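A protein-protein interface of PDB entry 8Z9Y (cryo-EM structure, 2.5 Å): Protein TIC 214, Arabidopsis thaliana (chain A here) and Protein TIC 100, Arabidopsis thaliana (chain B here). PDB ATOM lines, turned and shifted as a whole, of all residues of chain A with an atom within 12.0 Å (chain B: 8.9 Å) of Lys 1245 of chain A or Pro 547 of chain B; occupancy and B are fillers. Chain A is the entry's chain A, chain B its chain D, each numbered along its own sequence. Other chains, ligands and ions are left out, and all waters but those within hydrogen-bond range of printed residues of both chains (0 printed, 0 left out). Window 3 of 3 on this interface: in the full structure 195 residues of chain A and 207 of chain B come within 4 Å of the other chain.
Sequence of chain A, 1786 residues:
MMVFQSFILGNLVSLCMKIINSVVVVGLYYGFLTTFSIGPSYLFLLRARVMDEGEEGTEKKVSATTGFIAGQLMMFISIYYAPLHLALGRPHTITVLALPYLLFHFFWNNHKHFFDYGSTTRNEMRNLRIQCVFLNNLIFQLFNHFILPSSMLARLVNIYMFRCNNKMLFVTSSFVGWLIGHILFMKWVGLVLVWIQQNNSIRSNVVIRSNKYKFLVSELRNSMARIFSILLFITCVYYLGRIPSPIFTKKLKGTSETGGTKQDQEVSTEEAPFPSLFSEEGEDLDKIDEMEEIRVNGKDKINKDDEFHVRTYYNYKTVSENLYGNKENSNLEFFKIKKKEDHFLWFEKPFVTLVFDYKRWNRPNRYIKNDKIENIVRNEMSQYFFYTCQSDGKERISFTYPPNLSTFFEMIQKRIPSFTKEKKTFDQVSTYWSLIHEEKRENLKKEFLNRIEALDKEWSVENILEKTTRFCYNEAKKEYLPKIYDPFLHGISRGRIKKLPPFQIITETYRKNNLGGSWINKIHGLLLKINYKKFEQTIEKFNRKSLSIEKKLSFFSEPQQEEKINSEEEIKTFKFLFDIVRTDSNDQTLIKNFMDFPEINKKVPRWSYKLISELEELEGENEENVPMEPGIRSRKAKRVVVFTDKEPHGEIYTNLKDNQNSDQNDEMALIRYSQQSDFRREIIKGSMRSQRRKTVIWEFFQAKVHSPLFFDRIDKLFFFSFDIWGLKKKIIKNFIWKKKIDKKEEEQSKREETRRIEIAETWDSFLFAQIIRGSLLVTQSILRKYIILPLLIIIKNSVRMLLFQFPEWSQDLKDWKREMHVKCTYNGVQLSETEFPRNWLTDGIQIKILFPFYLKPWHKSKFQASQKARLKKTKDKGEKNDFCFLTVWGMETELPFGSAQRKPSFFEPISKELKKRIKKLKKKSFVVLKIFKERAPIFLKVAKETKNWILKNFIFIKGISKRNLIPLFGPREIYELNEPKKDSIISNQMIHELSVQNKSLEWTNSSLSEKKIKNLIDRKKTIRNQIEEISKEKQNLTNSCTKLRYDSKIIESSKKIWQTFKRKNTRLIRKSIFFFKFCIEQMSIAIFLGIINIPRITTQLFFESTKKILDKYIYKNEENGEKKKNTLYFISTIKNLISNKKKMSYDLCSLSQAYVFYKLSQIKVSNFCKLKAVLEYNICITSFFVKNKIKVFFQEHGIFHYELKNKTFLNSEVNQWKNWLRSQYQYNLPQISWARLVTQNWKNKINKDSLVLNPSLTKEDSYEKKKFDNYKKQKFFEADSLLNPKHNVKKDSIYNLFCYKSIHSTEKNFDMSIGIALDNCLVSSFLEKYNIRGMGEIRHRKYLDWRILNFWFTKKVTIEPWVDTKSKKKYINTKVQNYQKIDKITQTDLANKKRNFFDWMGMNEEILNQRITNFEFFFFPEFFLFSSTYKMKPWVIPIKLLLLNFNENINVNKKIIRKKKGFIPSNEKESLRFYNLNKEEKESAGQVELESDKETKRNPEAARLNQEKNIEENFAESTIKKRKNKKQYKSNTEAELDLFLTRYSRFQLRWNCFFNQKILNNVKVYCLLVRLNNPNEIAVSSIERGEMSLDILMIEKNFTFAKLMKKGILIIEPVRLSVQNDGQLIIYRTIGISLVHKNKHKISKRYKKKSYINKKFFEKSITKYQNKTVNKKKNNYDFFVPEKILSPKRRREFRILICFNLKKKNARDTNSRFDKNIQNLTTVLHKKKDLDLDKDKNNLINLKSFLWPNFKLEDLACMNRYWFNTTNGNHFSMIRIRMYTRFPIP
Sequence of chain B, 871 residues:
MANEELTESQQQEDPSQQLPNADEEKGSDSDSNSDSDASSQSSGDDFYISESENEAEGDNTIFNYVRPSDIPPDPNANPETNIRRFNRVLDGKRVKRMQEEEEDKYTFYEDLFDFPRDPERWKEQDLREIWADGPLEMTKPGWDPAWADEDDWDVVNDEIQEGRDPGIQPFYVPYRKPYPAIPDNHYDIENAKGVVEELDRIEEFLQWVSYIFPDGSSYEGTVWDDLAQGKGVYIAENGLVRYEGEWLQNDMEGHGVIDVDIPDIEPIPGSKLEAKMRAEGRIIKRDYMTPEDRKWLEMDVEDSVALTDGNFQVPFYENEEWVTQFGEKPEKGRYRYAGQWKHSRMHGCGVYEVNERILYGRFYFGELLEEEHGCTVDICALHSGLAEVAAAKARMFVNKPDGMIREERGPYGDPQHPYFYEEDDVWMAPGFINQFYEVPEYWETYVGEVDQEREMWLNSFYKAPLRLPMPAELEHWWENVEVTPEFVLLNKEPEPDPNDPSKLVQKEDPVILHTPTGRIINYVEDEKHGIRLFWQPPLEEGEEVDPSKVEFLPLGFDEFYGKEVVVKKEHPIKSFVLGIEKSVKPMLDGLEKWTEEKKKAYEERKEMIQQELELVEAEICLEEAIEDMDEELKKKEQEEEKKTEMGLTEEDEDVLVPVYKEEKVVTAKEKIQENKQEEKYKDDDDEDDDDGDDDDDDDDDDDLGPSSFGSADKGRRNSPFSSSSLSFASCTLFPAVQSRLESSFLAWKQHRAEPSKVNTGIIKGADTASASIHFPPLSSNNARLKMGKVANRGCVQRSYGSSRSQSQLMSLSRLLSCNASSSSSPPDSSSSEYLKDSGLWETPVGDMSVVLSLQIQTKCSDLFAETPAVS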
ATOM      1  N   TRP A1234      10.784  32.734  -6.328  1.00  0.00           N
ATOM      2  CA  TRP A1234      11.587  33.609  -5.480  1.00  0.00           C
ATOM      3  C   TRP A1234      12.663  32.847  -4.715  1.00  0.00           C
ATOM      4  O   TRP A1234      13.827  33.259  -4.694  1.00  0.00           O
ATOM      5  CB  TRP A1234      10.672  34.346  -4.498  1.00  0.00           C
ATOM      6  CG  TRP A1234      11.215  35.642  -3.985  1.00  0.00           C
ATOM      7  CD1 TRP A1234      12.526  36.004  -3.886  1.00  0.00           C
ATOM      8  CD2 TRP A1234      10.454  36.747  -3.482  1.00  0.00           C
ATOM      9  NE1 TRP A1234      12.629  37.270  -3.362  1.00  0.00           N
ATOM     10  CE2 TRP A1234      11.371  37.747  -3.103  1.00  0.00           C
ATOM     11  CE3 TRP A1234       9.087  36.989  -3.319  1.00  0.00           C
ATOM     12  CZ2 TRP A1234      10.964  38.970  -2.572  1.00  0.00           C
ATOM     13  CZ3 TRP A1234       8.685  38.202  -2.790  1.00  0.00           C
ATOM     14  CH2 TRP A1234       9.621  39.177  -2.423  1.00  0.00           C
ATOM     15  N   ALA A1235      12.284  31.735  -4.081  1.00  0.00           N
ATOM     16  CA  ALA A1235      13.243  30.976  -3.284  1.00  0.00           C
ATOM     17  C   ALA A1235      13.794  29.785  -4.062  1.00  0.00           C
ATOM     18  O   ALA A1235      14.937  29.367  -3.849  1.00  0.00           O
ATOM     19  CB  ALA A1235      12.592  30.515  -1.981  1.00  0.00           C
ATOM     20  N   ARG A1236      12.990  29.221  -4.961  1.00  0.00           N
ATOM     21  CA  ARG A1236      13.358  28.025  -5.708  1.00  0.00           C
ATOM     22  C   ARG A1236      14.531  28.307  -6.638  1.00  0.00           C
ATOM     23  O   ARG A1236      15.387  27.440  -6.844  1.00  0.00           O
ATOM     24  CB  ARG A1236      12.152  27.504  -6.495  1.00  0.00           C
ATOM     25  CG  ARG A1236      12.496  26.564  -7.635  1.00  0.00           C
ATOM     26  CD  ARG A1236      12.417  25.116  -7.179  1.00  0.00           C
ATOM     27  NE  ARG A1236      13.693  24.628  -6.667  1.00  0.00           N
ATOM     28  CZ  ARG A1236      13.836  23.533  -5.932  1.00  0.00           C
ATOM     29  NH1 ARG A1236      12.797  22.784  -5.599  1.00  0.00           N
ATOM     30  NH2 ARG A1236      15.051  23.182  -5.519  1.00  0.00           N
ATOM     31  N   LEU A1237      14.587  29.519  -7.199  1.00  0.00           N
ATOM     32  CA  LEU A1237      15.710  29.899  -8.047  1.00  0.00           C
ATOM     33  C   LEU A1237      17.020  29.867  -7.267  1.00  0.00           C
ATOM     34  O   LEU A1237      18.107  29.793  -7.850  1.00  0.00           O
ATOM     35  CB  LEU A1237      15.465  31.287  -8.644  1.00  0.00           C
ATOM     36  CG  LEU A1237      14.452  31.368  -9.788  1.00  0.00           C
ATOM     37  CD1 LEU A1237      14.015  32.806 -10.017  1.00  0.00           C
ATOM     38  CD2 LEU A1237      15.031  30.773 -11.061  1.00  0.00           C
ATOM     39  N   VAL A1238      16.932  29.941  -5.939  1.00  0.00           N
ATOM     40  CA  VAL A1238      18.112  29.941  -5.085  1.00  0.00           C
ATOM     41  C   VAL A1238      18.361  28.545  -4.522  1.00  0.00           C
ATOM     42  O   VAL A1238      19.505  28.175  -4.244  1.00  0.00           O
ATOM     43  CB  VAL A1238      17.969  30.972  -3.951  1.00  0.00           C
ATOM     44  CG1 VAL A1238      19.333  31.330  -3.388  1.00  0.00           C
ATOM     45  CG2 VAL A1238      17.249  32.215  -4.452  1.00  0.00           C
ATOM     46  N   THR A1239      17.300  27.761  -4.348  1.00  0.00           N
ATOM     47  CA  THR A1239      17.454  26.444  -3.734  1.00  0.00           C
ATOM     48  C   THR A1239      18.127  25.428  -4.654  1.00  0.00           C
ATOM     49  O   THR A1239      19.049  24.721  -4.231  1.00  0.00           O
ATOM     50  CB  THR A1239      16.101  25.891  -3.275  1.00  0.00           C
ATOM     51  OG1 THR A1239      15.227  25.754  -4.403  1.00  0.00           O
ATOM     52  CG2 THR A1239      15.469  26.792  -2.226  1.00  0.00           C
ATOM     53  N   GLN A1240      17.675  25.336  -5.906  1.00  0.00           N
ATOM     54  CA  GLN A1240      18.163  24.281  -6.793  1.00  0.00           C
ATOM     55  C   GLN A1240      19.646  24.442  -7.111  1.00  0.00           C
ATOM     56  O   GLN A1240      20.426  23.483  -7.015  1.00  0.00           O
ATOM     57  CB  GLN A1240      17.336  24.263  -8.080  1.00  0.00           C
ATOM     58  CG  GLN A1240      17.850  23.288  -9.127  1.00  0.00           C
ATOM     59  CD  GLN A1240      18.027  21.885  -8.579  1.00  0.00           C
ATOM     60  OE1 GLN A1240      19.135  21.351  -8.553  1.00  0.00           O
ATOM     61  NE2 GLN A1240      16.930  21.281  -8.137  1.00  0.00           N
ATOM     62  N   ASN A1241      20.051  25.656  -7.497  1.00  0.00           N
ATOM     63  CA  ASN A1241      21.460  25.906  -7.776  1.00  0.00           C
ATOM     64  C   ASN A1241      22.300  25.708  -6.522  1.00  0.00           C
ATOM     65  O   ASN A1241      23.439  25.244  -6.597  1.00  0.00           O
ATOM     66  CB  ASN A1241      21.657  27.306  -8.361  1.00  0.00           C
ATOM     67  CG  ASN A1241      20.947  28.366  -7.568  1.00  0.00           C
ATOM     68  OD1 ASN A1241      19.989  28.075  -6.866  1.00  0.00           O
ATOM     69  ND2 ASN A1241      21.410  29.605  -7.674  1.00  0.00           N
ATOM     70  N   TRP A1242      21.744  26.040  -5.354  1.00  0.00           N
ATOM     71  CA  TRP A1242      22.400  25.694  -4.096  1.00  0.00           C
ATOM     72  C   TRP A1242      22.676  24.197  -4.040  1.00  0.00           C
ATOM     73  O   TRP A1242      23.789  23.764  -3.712  1.00  0.00           O
ATOM     74  CB  TRP A1242      21.530  26.129  -2.913  1.00  0.00           C
ATOM     75  CG  TRP A1242      22.022  27.350  -2.193  1.00  0.00           C
ATOM     76  CD1 TRP A1242      21.562  28.627  -2.335  1.00  0.00           C
ATOM     77  CD2 TRP A1242      23.040  27.404  -1.188  1.00  0.00           C
ATOM     78  NE1 TRP A1242      22.244  29.475  -1.503  1.00  0.00           N
ATOM     79  CE2 TRP A1242      23.157  28.750  -0.785  1.00  0.00           C
ATOM     80  CE3 TRP A1242      23.874  26.450  -0.600  1.00  0.00           C
ATOM     81  CZ2 TRP A1242      24.070  29.163   0.178  1.00  0.00           C
ATOM     82  CZ3 TRP A1242      24.779  26.862   0.357  1.00  0.00           C
ATOM     83  CH2 TRP A1242      24.868  28.208   0.736  1.00  0.00           C
ATOM     84  N   LYS A1243      21.662  23.398  -4.385  1.00  0.00           N
ATOM     85  CA  LYS A1243      21.804  21.945  -4.411  1.00  0.00           C
ATOM     86  C   LYS A1243      22.978  21.517  -5.281  1.00  0.00           C
ATOM     87  O   LYS A1243      23.882  20.832  -4.794  1.00  0.00           O
ATOM     88  CB  LYS A1243      20.526  21.260  -4.911  1.00  0.00           C
ATOM     89  CG  LYS A1243      19.251  21.678  -4.213  1.00  0.00           C
ATOM     90  CD  LYS A1243      18.040  20.973  -4.808  1.00  0.00           C
ATOM     91  CE  LYS A1243      17.839  19.597  -4.196  1.00  0.00           C
ATOM     92  NZ  LYS A1243      17.002  19.654  -2.966  1.00  0.00           N
ATOM     93  N   ASN A1244      22.991  21.913  -6.560  1.00  0.00           N
ATOM     94  CA  ASN A1244      24.058  21.383  -7.418  1.00  0.00           C
ATOM     95  C   ASN A1244      25.422  21.954  -7.037  1.00  0.00           C
ATOM     96  O   ASN A1244      26.436  21.251  -7.124  1.00  0.00           O
ATOM     97  CB  ASN A1244      23.815  21.598  -8.920  1.00  0.00           C
ATOM     98  CG  ASN A1244      23.144  22.897  -9.247  1.00  0.00           C
ATOM     99  OD1 ASN A1244      22.037  23.150  -8.817  1.00  0.00           O
ATOM    100  ND2 ASN A1244      23.821  23.738 -10.020  1.00  0.00           N
ATOM    101  N   LYS A1245      25.479  23.222  -6.617  1.00  0.00           N
ATOM    102  CA  LYS A1245      26.762  23.805  -6.244  1.00  0.00           C
ATOM    103  C   LYS A1245      27.344  23.204  -4.972  1.00  0.00           C
ATOM    104  O   LYS A1245      28.568  23.250  -4.801  1.00  0.00           O
ATOM    105  CB  LYS A1245      26.646  25.324  -6.088  1.00  0.00           C
ATOM    106  CG  LYS A1245      26.226  26.060  -7.351  1.00  0.00           C
ATOM    107  CD  LYS A1245      27.090  25.674  -8.538  1.00  0.00           C
ATOM    108  CE  LYS A1245      26.680  26.441  -9.785  1.00  0.00           C
ATOM    109  NZ  LYS A1245      25.265  26.902  -9.712  1.00  0.00           N
ATOM    110  N   ILE A1246      26.525  22.649  -4.077  1.00  0.00           N
ATOM    111  CA  ILE A1246      27.052  21.931  -2.922  1.00  0.00           C
ATOM    112  C   ILE A1246      27.050  20.424  -3.118  1.00  0.00           C
ATOM    113  O   ILE A1246      27.465  19.696  -2.215  1.00  0.00           O
ATOM    114  CB  ILE A1246      26.306  22.295  -1.623  1.00  0.00           C
ATOM    115  CG1 ILE A1246      24.874  21.767  -1.653  1.00  0.00           C
ATOM    116  CG2 ILE A1246      26.337  23.802  -1.398  1.00  0.00           C
ATOM    117  CD1 ILE A1246      23.971  22.431  -0.649  1.00  0.00           C
ATOM    118  N   ASN A1247      26.591  19.927  -4.270  1.00  0.00           N
ATOM    119  CA  ASN A1247      26.713  18.501  -4.558  1.00  0.00           C
ATOM    120  C   ASN A1247      28.170  18.067  -4.643  1.00  0.00           C
ATOM    121  O   ASN A1247      28.517  16.972  -4.186  1.00  0.00           O
ATOM    122  CB  ASN A1247      25.983  18.157  -5.857  1.00  0.00           C
ATOM    123  CG  ASN A1247      24.492  17.969  -5.657  1.00  0.00           C
ATOM    124  OD1 ASN A1247      23.984  18.094  -4.544  1.00  0.00           O
ATOM    125  ND2 ASN A1247      23.784  17.669  -6.739  1.00  0.00           N
ATOM    126  N   LYS A1248      29.026  18.903  -5.229  1.00  0.00           N
ATOM    127  CA  LYS A1248      30.452  18.615  -5.379  1.00  0.00           C
ATOM    128  C   LYS A1248      30.682  17.322  -6.155  1.00  0.00           C
ATOM    129  O   LYS A1248      29.942  17.008  -7.088  1.00  0.00           O
ATOM    130  CB  LYS A1248      31.140  18.536  -4.010  1.00  0.00           C
ATOM    131  CG  LYS A1248      30.977  19.773  -3.134  1.00  0.00           C
ATOM    132  CD  LYS A1248      31.037  21.061  -3.942  1.00  0.00           C
ATOM    133  CE  LYS A1248      31.093  22.279  -3.034  1.00  0.00           C
ATOM    134  NZ  LYS A1248      30.287  22.088  -1.796  1.00  0.00           N
ATOM    135  N   VAL B 524      19.779  17.389   0.275  1.00  0.00           N
ATOM    136  CA  VAL B 524      20.395  16.703  -0.855  1.00  0.00           C
ATOM    137  C   VAL B 524      20.189  15.206  -0.667  1.00  0.00           C
ATOM    138  O   VAL B 524      19.592  14.774   0.324  1.00  0.00           O
ATOM    139  CB  VAL B 524      21.890  17.041  -0.987  1.00  0.00           C
ATOM    140  CG1 VAL B 524      22.085  18.532  -1.183  1.00  0.00           C
ATOM    141  CG2 VAL B 524      22.652  16.554   0.236  1.00  0.00           C
ATOM    142  N   PHE B 534      20.139  20.464   5.066  1.00  0.00           N
ATOM    143  CA  PHE B 534      21.067  21.512   5.459  1.00  0.00           C
ATOM    144  C   PHE B 534      20.312  22.824   5.608  1.00  0.00           C
ATOM    145  O   PHE B 534      19.176  22.970   5.152  1.00  0.00           O
ATOM    146  CB  PHE B 534      22.191  21.668   4.433  1.00  0.00           C
ATOM    147  CG  PHE B 534      21.696  21.901   3.034  1.00  0.00           C
ATOM    148  CD1 PHE B 534      21.410  20.833   2.203  1.00  0.00           C
ATOM    149  CD2 PHE B 534      21.492  23.184   2.561  1.00  0.00           C
ATOM    150  CE1 PHE B 534      20.943  21.043   0.924  1.00  0.00           C
ATOM    151  CE2 PHE B 534      21.029  23.398   1.281  1.00  0.00           C
ATOM    152  CZ  PHE B 534      20.752  22.325   0.462  1.00  0.00           C
ATOM    153  N   GLN B 536      19.710  26.645   4.589  1.00  0.00           N
ATOM    154  CA  GLN B 536      19.868  27.468   3.399  1.00  0.00           C
ATOM    155  C   GLN B 536      20.044  28.916   3.838  1.00  0.00           C
ATOM    156  O   GLN B 536      19.093  29.507   4.373  1.00  0.00           O
ATOM    157  CB  GLN B 536      18.661  27.323   2.483  1.00  0.00           C
ATOM    158  CG  GLN B 536      18.571  28.364   1.385  1.00  0.00           C
ATOM    159  CD  GLN B 536      18.927  27.805   0.025  1.00  0.00           C
ATOM    160  OE1 GLN B 536      19.445  26.694  -0.086  1.00  0.00           O
ATOM    161  NE2 GLN B 536      18.650  28.573  -1.021  1.00  0.00           N
ATOM    162  N   PRO B 537      21.226  29.508   3.678  1.00  0.00           N
ATOM    163  CA  PRO B 537      21.450  30.886   4.151  1.00  0.00           C
ATOM    164  C   PRO B 537      20.491  31.886   3.522  1.00  0.00           C
ATOM    165  O   PRO B 537      20.024  32.801   4.216  1.00  0.00           O
ATOM    166  CB  PRO B 537      22.908  31.162   3.748  1.00  0.00           C
ATOM    167  CG  PRO B 537      23.543  29.813   3.754  1.00  0.00           C
ATOM    168  CD  PRO B 537      22.481  28.850   3.280  1.00  0.00           C
ATOM    169  N   PRO B 538      20.157  31.768   2.212  1.00  0.00           N
ATOM    170  CA  PRO B 538      19.083  32.622   1.685  1.00  0.00           C
ATOM    171  C   PRO B 538      17.716  32.185   2.185  1.00  0.00           C
ATOM    172  O   PRO B 538      17.568  31.065   2.677  1.00  0.00           O
ATOM    173  CB  PRO B 538      19.209  32.457   0.164  1.00  0.00           C
ATOM    174  CG  PRO B 538      20.597  31.984  -0.050  1.00  0.00           C
ATOM    175  CD  PRO B 538      20.865  31.092   1.110  1.00  0.00           C
ATOM    176  N   GLU B 544      19.821  36.247  -1.585  1.00  0.00           N
ATOM    177  CA  GLU B 544      20.449  35.622  -2.745  1.00  0.00           C
ATOM    178  C   GLU B 544      21.966  35.786  -2.745  1.00  0.00           C
ATOM    179  O   GLU B 544      22.562  36.061  -1.698  1.00  0.00           O
ATOM    180  CB  GLU B 544      19.831  36.187  -4.034  1.00  0.00           C
ATOM    181  CG  GLU B 544      20.319  37.575  -4.465  1.00  0.00           C
ATOM    182  CD  GLU B 544      19.749  38.710  -3.631  1.00  0.00           C
ATOM    183  OE1 GLU B 544      19.984  39.883  -3.992  1.00  0.00           O
ATOM    184  OE2 GLU B 544      19.058  38.442  -2.627  1.00  0.00           O
ATOM    185  N   VAL B 545      22.585  35.548  -3.911  1.00  0.00           N
ATOM    186  CA  VAL B 545      23.997  35.776  -4.243  1.00  0.00           C
ATOM    187  C   VAL B 545      24.830  34.528  -3.967  1.00  0.00           C
ATOM    188  O   VAL B 545      25.422  34.383  -2.891  1.00  0.00           O
ATOM    189  CB  VAL B 545      24.599  37.007  -3.531  1.00  0.00           C
ATOM    190  CG1 VAL B 545      26.043  37.214  -3.965  1.00  0.00           C
ATOM    191  CG2 VAL B 545      23.796  38.262  -3.848  1.00  0.00           C
ATOM    192  N   ASP B 546      24.858  33.618  -4.949  1.00  0.00           N
ATOM    193  CA  ASP B 546      25.803  32.519  -5.151  1.00  0.00           C
ATOM    194  C   ASP B 546      25.878  31.503  -4.014  1.00  0.00           C
ATOM    195  O   ASP B 546      26.062  31.869  -2.846  1.00  0.00           O
ATOM    196  CB  ASP B 546      27.200  33.090  -5.406  1.00  0.00           C
ATOM    197  CG  ASP B 546      28.293  32.055  -5.228  1.00  0.00           C
ATOM    198  OD1 ASP B 546      28.952  32.058  -4.167  1.00  0.00           O
ATOM    199  OD2 ASP B 546      28.495  31.238  -6.151  1.00  0.00           O
ATOM    200  N   PRO B 547      25.765  30.211  -4.326  1.00  0.00           N
ATOM    201  CA  PRO B 547      26.038  29.172  -3.325  1.00  0.00           C
ATOM    202  C   PRO B 547      27.486  28.706  -3.355  1.00  0.00           C
ATOM    203  O   PRO B 547      27.976  28.301  -4.414  1.00  0.00           O
ATOM    204  CB  PRO B 547      25.084  28.040  -3.729  1.00  0.00           C
ATOM    205  CG  PRO B 547      24.457  28.472  -5.071  1.00  0.00           C
ATOM    206  CD  PRO B 547      25.252  29.629  -5.573  1.00  0.00           C
ATOM    207  N   SER B 548      28.185  28.746  -2.219  1.00  0.00           N
ATOM    208  CA  SER B 548      29.552  28.240  -2.196  1.00  0.00           C
ATOM    209  C   SER B 548      29.803  27.254  -1.061  1.00  0.00           C
ATOM    210  O   SER B 548      30.453  26.224  -1.265  1.00  0.00           O
ATOM    211  CB  SER B 548      30.540  29.406  -2.097  1.00  0.00           C
ATOM    212  OG  SER B 548      30.001  30.464  -1.324  1.00  0.00           O
ATOM    213  N   LYS B 549      29.268  27.538   0.123  1.00  0.00           N
ATOM    214  CA  LYS B 549      29.516  26.743   1.318  1.00  0.00           C
ATOM    215  C   LYS B 549      28.222  26.510   2.090  1.00  0.00           C
ATOM    216  O   LYS B 549      27.328  27.356   2.128  1.00  0.00           O
ATOM    217  CB  LYS B 549      30.556  27.424   2.218  1.00  0.00           C
ATOM    218  CG  LYS B 549      31.996  27.370   1.712  1.00  0.00           C
ATOM    219  CD  LYS B 549      32.365  26.005   1.143  1.00  0.00           C
ATOM    220  CE  LYS B 549      32.377  24.926   2.220  1.00  0.00           C
ATOM    221  NZ  LYS B 549      32.479  23.560   1.636  1.00  0.00           N
ATOM    222  N   VAL B 550      28.149  25.353   2.745  1.00  0.00           N
ATOM    223  CA  VAL B 550      26.908  24.892   3.358  1.00  0.00           C
ATOM    224  C   VAL B 550      27.116  24.716   4.859  1.00  0.00           C
ATOM    225  O   VAL B 550      28.238  24.849   5.359  1.00  0.00           O
ATOM    226  CB  VAL B 550      26.440  23.585   2.689  1.00  0.00           C
ATOM    227  CG1 VAL B 550      27.244  22.404   3.207  1.00  0.00           C
ATOM    228  CG2 VAL B 550      24.944  23.377   2.865  1.00  0.00           C
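Of the 15 printed residues of chain A, 7 touch a printed residue of chain B. Printed residues of chain A that touch a printed residue of chain B: Val 1238, Thr 1239, Asn 1241, Trp 1242, Lys 1245, Ile 1246 and Asn 1247. Hydrophobic or aromatic side chains of chain A within 4 Å of the printed part of chain B: Val 1238, Trp 1242 and Ile 1246. Hydrophobic or aromatic side chains of chain B that line the printed part of chain A: Val 524, Phe 534, Pro 537, Pro 538, Pro 547 and Val 550. Among the printed residues, 13 pairs touch across the chains. Among the printed residues, no Asp or Glu carboxylate lies within 4 Å of a Lys or Arg side-chain nitrogen of the other chain.
The guanidinium group of Arg 1236 of chain A is in hydrogen-bond range of the side-chain hydroxyl of Thr 1239 of chain A (2.8 Å). The backbone carbonyl oxygen (O) of Leu 1237 of chain A sits close to the side-chain amide oxygen (OD1) of Asn 1241 of chain A (2.7 Å). The backbone carbonyl oxygen (O) of Val 1238 of chain A lies close to the side-chain amide oxygen (OD1) of Asn 1241 of chain A (2.7 Å). The side-chain amide oxygen of Asn 1244 of chain A sits close to the backbone carbonyl oxygen of Asn 1241 of chain A. The backbone carbonyl oxygen of Lys 1243 of chain A sits close to the side-chain amide oxygen of Asn 1247 of chain A. ND2 of Asn 1244 of chain A lies close to NZ of Lys 1245 of chain A.
Of the printed residues of chain B, Trp 1242 of chain A touches Gln 536 (3.2 Å), Pro 537 (3.5 Å), Pro 538 (3.3 Å), Pro 547 (3.3 Å) and Lys 549 (3.0 Å). Lys 1243 of chain A touches none of the printed residues of chain B. No residue of chain B comes within 4 Å of Asn 1244 of chain A. Lys 1245 of chain A touches just one residue of chain B: Pro 547. Of the printed residues of chain B, Asn 1247 of chain A touches Val 524. Of the printed residues of chain A, Val 524 of chain B touches Asn 1247 (3.9 Å). No residue of chain A comes within 4 Å of Asp 546 of chain B. Pro 547 of chain B touches three residues of chain A. No residue of chain A comes within 4 Å of Ser 548 of chain B. The nearest residue of chain B that does not touch Lys 1245 of chain A is Ser 548 of chain B (5.0 Å). The nearest residue of chain A that does not touch Pro 547 of chain B is Ile 1246 of chain A (5.0 Å).
The side-chain amide nitrogen (NE2) of Gln 536 of chain B is in hydrogen-bond range of the backbone carbonyl oxygen (O) of Val 1238 of chain A (3.4 Å).
Among the printed residues, pairs that only touch across the chains: Trp 1242 of chain A with Lys 549 of chain B, Trp 1242 of chain A with Gln 536 of chain B, Trp 1242 of chain A with Pro 547 of chain B, Trp 1242 of chain A with Pro 538 of chain B, Ile 1246 of chain A with Phe 534 of chain B, Trp 1242 of chain A with Pro 537 of chain B, Val 1238 of chain A with Pro 538 of chain B, Thr 1239 of chain A with Gln 536 of chain B, Lys 1245 of chain A with Pro 547 of chain B, Asn 1241 of chain A with Pro 547 of chain B, Ile 1246 of chain A with Val 550 of chain B and Asn 1247 of chain A with Val 524 of chain B.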
